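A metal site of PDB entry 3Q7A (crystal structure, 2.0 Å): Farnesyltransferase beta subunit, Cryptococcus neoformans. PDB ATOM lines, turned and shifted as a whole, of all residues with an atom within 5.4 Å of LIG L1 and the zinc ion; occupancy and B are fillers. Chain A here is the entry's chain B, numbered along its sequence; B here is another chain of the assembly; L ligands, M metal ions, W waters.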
ATOM      1  N   LEU A  84      -4.675   4.780   1.539  1.00  0.00           N
ATOM      2  CA  LEU A  84      -4.939   3.949   0.367  1.00  0.00           C
ATOM      3  C   LEU A  84      -3.690   3.218  -0.145  1.00  0.00           C
ATOM      4  O   LEU A  84      -3.654   2.766  -1.296  1.00  0.00           O
ATOM      5  CB  LEU A  84      -5.574   4.786  -0.763  1.00  0.00           C
ATOM      6  CG  LEU A  84      -6.963   5.375  -0.513  1.00  0.00           C
ATOM      7  CD1 LEU A  84      -7.302   6.410  -1.574  1.00  0.00           C
ATOM      8  CD2 LEU A  84      -8.021   4.279  -0.454  1.00  0.00           C
ATOM      9  N   SER A  87      -4.322  -0.004  -1.516  1.00  0.00           N
ATOM     10  CA  SER A  87      -5.277   0.101  -2.616  1.00  0.00           C
ATOM     11  C   SER A  87      -4.722   0.808  -3.858  1.00  0.00           C
ATOM     12  O   SER A  87      -5.490   1.320  -4.675  1.00  0.00           O
ATOM     13  CB  SER A  87      -6.552   0.815  -2.149  1.00  0.00           C
ATOM     14  OG  SER A  87      -7.279   0.002  -1.254  1.00  0.00           O
ATOM     15  N   TRP A  90      -6.134   0.143  -7.289  1.00  0.00           N
ATOM     16  CA  TRP A  90      -7.424   0.806  -7.497  1.00  0.00           C
ATOM     17  C   TRP A  90      -7.241   2.239  -7.963  1.00  0.00           C
ATOM     18  O   TRP A  90      -7.964   2.704  -8.838  1.00  0.00           O
ATOM     19  CB  TRP A  90      -8.283   0.762  -6.230  1.00  0.00           C
ATOM     20  CG  TRP A  90      -8.900  -0.584  -5.973  1.00  0.00           C
ATOM     21  CD1 TRP A  90      -8.522  -1.484  -5.020  1.00  0.00           C
ATOM     22  CD2 TRP A  90      -9.996  -1.175  -6.684  1.00  0.00           C
ATOM     23  NE1 TRP A  90      -9.324  -2.604  -5.094  1.00  0.00           N
ATOM     24  CE2 TRP A  90     -10.225  -2.442  -6.104  1.00  0.00           C
ATOM     25  CE3 TRP A  90     -10.806  -0.763  -7.758  1.00  0.00           C
ATOM     26  CZ2 TRP A  90     -11.239  -3.297  -6.564  1.00  0.00           C
ATOM     27  CZ3 TRP A  90     -11.801  -1.613  -8.209  1.00  0.00           C
ATOM     28  CH2 TRP A  90     -12.013  -2.873  -7.605  1.00  0.00           C
ATOM     29  N   TRP A  94      -8.940   3.309 -11.295  1.00  0.00           N
ATOM     30  CA  TRP A  94      -9.841   4.458 -11.309  1.00  0.00           C
ATOM     31  C   TRP A  94      -9.397   5.515 -12.313  1.00  0.00           C
ATOM     32  O   TRP A  94     -10.216   6.100 -13.006  1.00  0.00           O
ATOM     33  CB  TRP A  94     -10.006   5.084  -9.911  1.00  0.00           C
ATOM     34  CG  TRP A  94     -10.677   4.180  -8.888  1.00  0.00           C
ATOM     35  CD1 TRP A  94     -11.686   3.282  -9.114  1.00  0.00           C
ATOM     36  CD2 TRP A  94     -10.381   4.118  -7.490  1.00  0.00           C
ATOM     37  NE1 TRP A  94     -12.034   2.652  -7.938  1.00  0.00           N
ATOM     38  CE2 TRP A  94     -11.249   3.152  -6.926  1.00  0.00           C
ATOM     39  CE3 TRP A  94      -9.470   4.777  -6.657  1.00  0.00           C
ATOM     40  CZ2 TRP A  94     -11.224   2.828  -5.560  1.00  0.00           C
ATOM     41  CZ3 TRP A  94      -9.453   4.460  -5.300  1.00  0.00           C
ATOM     42  CH2 TRP A  94     -10.326   3.490  -4.767  1.00  0.00           C
ATOM     43  N   LEU A 141      -9.018  -8.415  -4.645  1.00  0.00           N
ATOM     44  CA  LEU A 141      -9.484  -7.119  -5.148  1.00  0.00           C
ATOM     45  C   LEU A 141      -8.453  -6.354  -6.005  1.00  0.00           C
ATOM     46  O   LEU A 141      -8.784  -5.924  -7.109  1.00  0.00           O
ATOM     47  CB  LEU A 141     -10.061  -6.259  -4.013  1.00  0.00           C
ATOM     48  CG  LEU A 141     -11.523  -6.520  -3.611  1.00  0.00           C
ATOM     49  CD1 LEU A 141     -11.807  -7.988  -3.247  1.00  0.00           C
ATOM     50  CD2 LEU A 141     -11.952  -5.613  -2.464  1.00  0.00           C
ATOM     51  N   ARG A 197     -17.567  -9.359  -2.865  1.00  0.00           N
ATOM     52  CA  ARG A 197     -16.529  -8.595  -3.584  1.00  0.00           C
ATOM     53  C   ARG A 197     -15.421  -9.525  -4.048  1.00  0.00           C
ATOM     54  O   ARG A 197     -14.948  -9.433  -5.176  1.00  0.00           O
ATOM     55  CB  ARG A 197     -15.918  -7.496  -2.704  1.00  0.00           C
ATOM     56  CG  ARG A 197     -16.866  -6.413  -2.202  1.00  0.00           C
ATOM     57  CD  ARG A 197     -16.165  -5.543  -1.157  1.00  0.00           C
ATOM     58  NE  ARG A 197     -15.545  -6.369  -0.111  1.00  0.00           N
ATOM     59  CZ  ARG A 197     -14.457  -6.048   0.585  1.00  0.00           C
ATOM     60  NH1 ARG A 197     -13.837  -4.897   0.380  1.00  0.00           N
ATOM     61  NH2 ARG A 197     -13.992  -6.889   1.503  1.00  0.00           N
ATOM     62  N   ASP A 323     -25.881   8.890  -3.865  1.00  0.00           N
ATOM     63  CA  ASP A 323     -24.432   9.000  -3.964  1.00  0.00           C
ATOM     64  C   ASP A 323     -24.015   8.653  -5.386  1.00  0.00           C
ATOM     65  O   ASP A 323     -24.393   7.601  -5.908  1.00  0.00           O
ATOM     66  CB  ASP A 323     -23.761   8.072  -2.950  1.00  0.00           C
ATOM     67  CG  ASP A 323     -22.241   8.072  -3.017  1.00  0.00           C
ATOM     68  OD1 ASP A 323     -21.645   8.496  -4.031  1.00  0.00           O
ATOM     69  OD2 ASP A 323     -21.615   7.629  -2.029  1.00  0.00           O
ATOM     70  N   GLY A 324     -23.244   9.542  -5.992  1.00  0.00           N
ATOM     71  CA  GLY A 324     -22.776   9.391  -7.365  1.00  0.00           C
ATOM     72  C   GLY A 324     -22.126   8.066  -7.717  1.00  0.00           C
ATOM     73  O   GLY A 324     -22.250   7.594  -8.851  1.00  0.00           O
ATOM     74  N   CYS A 325     -21.416   7.454  -6.773  1.00  0.00           N
ATOM     75  CA  CYS A 325     -20.725   6.189  -7.072  1.00  0.00           C
ATOM     76  C   CYS A 325     -21.690   5.041  -7.360  1.00  0.00           C
ATOM     77  O   CYS A 325     -21.338   4.108  -8.084  1.00  0.00           O
ATOM     78  CB  CYS A 325     -19.707   5.808  -5.982  1.00  0.00           C
ATOM     79  SG  CYS A 325     -20.394   5.317  -4.380  1.00  0.00           S
ATOM     80  N   TYR A 326     -22.910   5.116  -6.821  1.00  0.00           N
ATOM     81  CA  TYR A 326     -23.923   4.076  -7.035  1.00  0.00           C
ATOM     82  C   TYR A 326     -24.550   4.118  -8.426  1.00  0.00           C
ATOM     83  O   TYR A 326     -25.341   3.241  -8.777  1.00  0.00           O
ATOM     84  CB  TYR A 326     -24.980   4.100  -5.925  1.00  0.00           C
ATOM     85  CG  TYR A 326     -24.368   3.851  -4.569  1.00  0.00           C
ATOM     86  CD1 TYR A 326     -23.571   2.735  -4.337  1.00  0.00           C
ATOM     87  CD2 TYR A 326     -24.564   4.751  -3.526  1.00  0.00           C
ATOM     88  CE1 TYR A 326     -22.974   2.512  -3.105  1.00  0.00           C
ATOM     89  CE2 TYR A 326     -23.979   4.532  -2.282  1.00  0.00           C
ATOM     90  CZ  TYR A 326     -23.188   3.411  -2.079  1.00  0.00           C
ATOM     91  OH  TYR A 326     -22.611   3.183  -0.855  1.00  0.00           O
ATOM     92  N   TRP A 329     -22.591   1.126  -9.335  1.00  0.00           N
ATOM     93  CA  TRP A 329     -22.925  -0.076  -8.563  1.00  0.00           C
ATOM     94  C   TRP A 329     -24.379  -0.510  -8.716  1.00  0.00           C
ATOM     95  O   TRP A 329     -24.658  -1.694  -8.914  1.00  0.00           O
ATOM     96  CB  TRP A 329     -22.542   0.057  -7.081  1.00  0.00           C
ATOM     97  CG  TRP A 329     -21.091   0.400  -6.867  1.00  0.00           C
ATOM     98  CD1 TRP A 329     -20.603   1.539  -6.318  1.00  0.00           C
ATOM     99  CD2 TRP A 329     -19.957  -0.397  -7.244  1.00  0.00           C
ATOM    100  NE1 TRP A 329     -19.224   1.512  -6.306  1.00  0.00           N
ATOM    101  CE2 TRP A 329     -18.803   0.339  -6.865  1.00  0.00           C
ATOM    102  CE3 TRP A 329     -19.798  -1.654  -7.847  1.00  0.00           C
ATOM    103  CZ2 TRP A 329     -17.506  -0.148  -7.082  1.00  0.00           C
ATOM    104  CZ3 TRP A 329     -18.499  -2.127  -8.066  1.00  0.00           C
ATOM    105  CH2 TRP A 329     -17.373  -1.370  -7.680  1.00  0.00           C
ATOM    106  N   ASP A 400     -19.266  12.215  -4.579  1.00  0.00           N
ATOM    107  CA  ASP A 400     -20.405  11.588  -3.930  1.00  0.00           C
ATOM    108  C   ASP A 400     -21.669  12.445  -4.121  1.00  0.00           C
ATOM    109  O   ASP A 400     -22.630  12.017  -4.757  1.00  0.00           O
ATOM    110  CB  ASP A 400     -20.052  11.400  -2.441  1.00  0.00           C
ATOM    111  CG  ASP A 400     -21.239  11.069  -1.551  1.00  0.00           C
ATOM    112  OD1 ASP A 400     -22.396  10.950  -2.027  1.00  0.00           O
ATOM    113  OD2 ASP A 400     -20.994  10.934  -0.342  1.00  0.00           O
ATOM    114  N   TYR A 409     -12.005   7.471  -6.849  1.00  0.00           N
ATOM    115  CA  TYR A 409     -13.050   6.455  -6.731  1.00  0.00           C
ATOM    116  C   TYR A 409     -14.403   6.961  -7.252  1.00  0.00           C
ATOM    117  O   TYR A 409     -15.058   6.278  -8.043  1.00  0.00           O
ATOM    118  CB  TYR A 409     -13.167   5.975  -5.274  1.00  0.00           C
ATOM    119  CG  TYR A 409     -14.442   5.222  -4.963  1.00  0.00           C
ATOM    120  CD1 TYR A 409     -14.580   3.868  -5.290  1.00  0.00           C
ATOM    121  CD2 TYR A 409     -15.516   5.865  -4.351  1.00  0.00           C
ATOM    122  CE1 TYR A 409     -15.758   3.172  -5.012  1.00  0.00           C
ATOM    123  CE2 TYR A 409     -16.701   5.185  -4.077  1.00  0.00           C
ATOM    124  CZ  TYR A 409     -16.806   3.845  -4.410  1.00  0.00           C
ATOM    125  OH  TYR A 409     -17.979   3.177  -4.136  1.00  0.00           O
ATOM    126  N   HIS A 410     -14.806   8.158  -6.833  1.00  0.00           N
ATOM    127  CA  HIS A 410     -16.067   8.713  -7.308  1.00  0.00           C
ATOM    128  C   HIS A 410     -16.016   9.178  -8.756  1.00  0.00           C
ATOM    129  O   HIS A 410     -17.013   9.108  -9.466  1.00  0.00           O
ATOM    130  CB  HIS A 410     -16.573   9.819  -6.370  1.00  0.00           C
ATOM    131  CG  HIS A 410     -17.185   9.291  -5.120  1.00  0.00           C
ATOM    132  ND1 HIS A 410     -16.470   9.176  -3.942  1.00  0.00           N
ATOM    133  CD2 HIS A 410     -18.420   8.806  -4.861  1.00  0.00           C
ATOM    134  CE1 HIS A 410     -17.261   8.657  -3.011  1.00  0.00           C
ATOM    135  NE2 HIS A 410     -18.436   8.423  -3.547  1.00  0.00           N
ATOM    136  N   TYR B 123     -12.504  -2.682   7.022  1.00  0.00           N
ATOM    137  CA  TYR B 123     -12.839  -4.101   6.883  1.00  0.00           C
ATOM    138  C   TYR B 123     -11.918  -4.948   7.772  1.00  0.00           C
ATOM    139  O   TYR B 123     -12.369  -5.903   8.421  1.00  0.00           O
ATOM    140  CB  TYR B 123     -12.640  -4.558   5.436  1.00  0.00           C
ATOM    141  CG  TYR B 123     -13.792  -4.289   4.494  1.00  0.00           C
ATOM    142  CD1 TYR B 123     -14.840  -5.201   4.359  1.00  0.00           C
ATOM    143  CD2 TYR B 123     -13.823  -3.132   3.716  1.00  0.00           C
ATOM    144  CE1 TYR B 123     -15.906  -4.958   3.485  1.00  0.00           C
ATOM    145  CE2 TYR B 123     -14.876  -2.885   2.835  1.00  0.00           C
ATOM    146  CZ  TYR B 123     -15.909  -3.802   2.726  1.00  0.00           C
ATOM    147  OH  TYR B 123     -16.955  -3.562   1.856  1.00  0.00           O
HETATM  148  N1  LIG L   1     -15.496   4.104   0.459  1.00  0.00           N
HETATM  149  C1  LIG L   1     -14.682   4.860  -0.515  1.00  0.00           C
HETATM  150  C2  LIG L   1     -16.454   4.986   1.142  1.00  0.00           C
HETATM  151  C3  LIG L   1     -14.603   3.383   1.378  1.00  0.00           C
HETATM  152  C4  LIG L   1     -14.063   3.875  -1.526  1.00  0.00           C
HETATM  153  C5  LIG L   1     -17.655   5.198   0.197  1.00  0.00           C
HETATM  154  C6  LIG L   1     -13.745   2.414   0.543  1.00  0.00           C
HETATM  155  N2  LIG L   1     -13.492   2.672  -0.829  1.00  0.00           N
HETATM  156  N3  LIG L   1     -18.690   4.393   0.015  1.00  0.00           N
HETATM  157  C7  LIG L   1     -17.831   6.230  -0.621  1.00  0.00           C
HETATM  158  O1  LIG L   1     -13.280   1.414   1.077  1.00  0.00           O
HETATM  159  C8  LIG L   1     -12.727   1.765  -1.608  1.00  0.00           C
HETATM  160  C9  LIG L   1     -18.941   3.130   0.730  1.00  0.00           C
HETATM  161  C10 LIG L   1     -19.525   4.903  -0.884  1.00  0.00           C
HETATM  162  N4  LIG L   1     -18.974   6.054  -1.295  1.00  0.00           N
HETATM  163  C11 LIG L   1     -13.361   1.082  -2.643  1.00  0.00           C
HETATM  164  C12 LIG L   1     -11.374   1.555  -1.369  1.00  0.00           C
HETATM  165  C13 LIG L   1     -18.008   1.984   0.318  1.00  0.00           C
HETATM  166  C14 LIG L   1     -12.644   0.182  -3.431  1.00  0.00           C
HETATM  167  C15 LIG L   1     -10.647   0.654  -2.155  1.00  0.00           C
HETATM  168  C16 LIG L   1     -17.551   1.105   1.307  1.00  0.00           C
HETATM  169  C17 LIG L   1     -17.636   1.792  -1.009  1.00  0.00           C
HETATM  170  C18 LIG L   1     -11.294  -0.042  -3.189  1.00  0.00           C
HETATM  171 CL1  LIG L   1     -13.462  -0.641  -4.713  1.00  0.00          CL
HETATM  172  C19 LIG L   1     -16.709   0.054   0.974  1.00  0.00           C
HETATM  173  C20 LIG L   1     -16.796   0.727  -1.341  1.00  0.00           C
HETATM  174  C21 LIG L   1     -16.337  -0.138  -0.354  1.00  0.00           C
HETATM  175  C22 LIG L   1     -15.478  -1.230  -0.699  1.00  0.00           C
HETATM  176  N5  LIG L   1     -14.781  -2.093  -0.981  1.00  0.00           N
HETATM  177  C1  LG2 L   2     -21.419   0.793   3.144  1.00  0.00           C
HETATM  178  O1  LG2 L   2     -20.644   1.992   3.264  1.00  0.00           O
HETATM  179  C2  LG2 L   2     -20.948   0.003   2.090  1.00  0.00           C
HETATM  180  C3  LG2 L   2     -20.170  -1.161   2.146  1.00  0.00           C
HETATM  181  C4  LG2 L   2     -19.706  -1.719   3.497  1.00  0.00           C
HETATM  182  C5  LG2 L   2     -19.752  -1.934   0.878  1.00  0.00           C
HETATM  183  C6  LG2 L   2     -19.869  -1.141  -0.439  1.00  0.00           C
HETATM  184  C7  LG2 L   2     -19.425  -1.890  -1.534  1.00  0.00           C
HETATM  185  C8  LG2 L   2     -19.217  -1.453  -2.845  1.00  0.00           C
HETATM  186  C9  LG2 L   2     -19.554  -0.005  -3.257  1.00  0.00           C
HETATM  187  C10 LG2 L   2     -18.783  -2.413  -3.952  1.00  0.00           C
HETATM  188  C11 LG2 L   2     -17.395  -3.030  -3.797  1.00  0.00           C
HETATM  189  C12 LG2 L   2     -17.052  -3.668  -4.992  1.00  0.00           C
HETATM  190  C13 LG2 L   2     -15.790  -4.121  -5.395  1.00  0.00           C
HETATM  191  C14 LG2 L   2     -14.577  -3.955  -4.484  1.00  0.00           C
HETATM  192  C15 LG2 L   2     -15.629  -4.798  -6.755  1.00  0.00           C
HETATM  193  P1  LG2 L   2     -21.268   3.406   3.785  1.00  0.00           P
HETATM  194  O2  LG2 L   2     -22.184   3.176   4.920  1.00  0.00           O
HETATM  195  O3  LG2 L   2     -20.122   4.319   3.948  1.00  0.00           O
HETATM  196  O4  LG2 L   2     -22.100   3.892   2.483  1.00  0.00           O
HETATM  197  P2  LG2 L   2     -23.722   4.061   2.402  1.00  0.00           P
HETATM  198  O5  LG2 L   2     -24.258   5.058   3.357  1.00  0.00           O
HETATM  199  O6  LG2 L   2     -24.381   2.622   2.584  1.00  0.00           O
HETATM  200  O7  LG2 L   2     -23.976   4.457   0.873  1.00  0.00           O
HETATM  201 ZN    ZN M   1     -19.813   7.044  -2.948  1.00  0.00          ZN
HETATM  202  O   HOH W   1     -11.279  -0.731   1.277  1.00  0.00           O
HETATM  203  O   HOH W   2     -13.725   0.803   3.624  1.00  0.00           O
HETATM  204  O   HOH W   3     -20.184   6.581   2.292  1.00  0.00           O
HETATM  205  O   HOH W   4     -14.600   8.120  -1.352  1.00  0.00           O
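A nitrogen (N5) of LIG L1 is in hydrogen-bond range of the guanidinium group of Arg 197 (3.3 Å). The side-chain hydroxyl (OH) of Tyr 326 sits at hydrogen-bond distance from an oxygen (O7) of LG2 L2 (2.5 Å).
OH of Tyr 409 sits close to SG of Cys 325, at 3.2 Å. OH of Tyr 409 lies within hydrogen-bond range of NE1 of Trp 329.
Merely in contact with LIG L1: Tyr 409, Tyr 326, Ser 87, Trp 90, Trp 94 and Tyr 123 of chain B. Hydrophobic or aromatic side chains within 4 Å of LIG L1: Trp 90, Trp 94, Tyr 409, His 410 and Tyr 123 of chain B. Of the 15 residues printed, 10 come within 4 Å of LIG L1. The nearest printed residue that does not touch LIG L1 is Leu 84 (4.4 Å).
Tyr 409 touches the zinc ion (CE2 to ZN, 3.8 Å). The nearest printed residue that does not touch the zinc ion is Asp 400 (4.4 Å).
The zinc ion is bound by NE2 of His 410, N4 of LIG L1, OD2 of Asp 323, SG of Cys 325 and OD1 of Asp 323.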
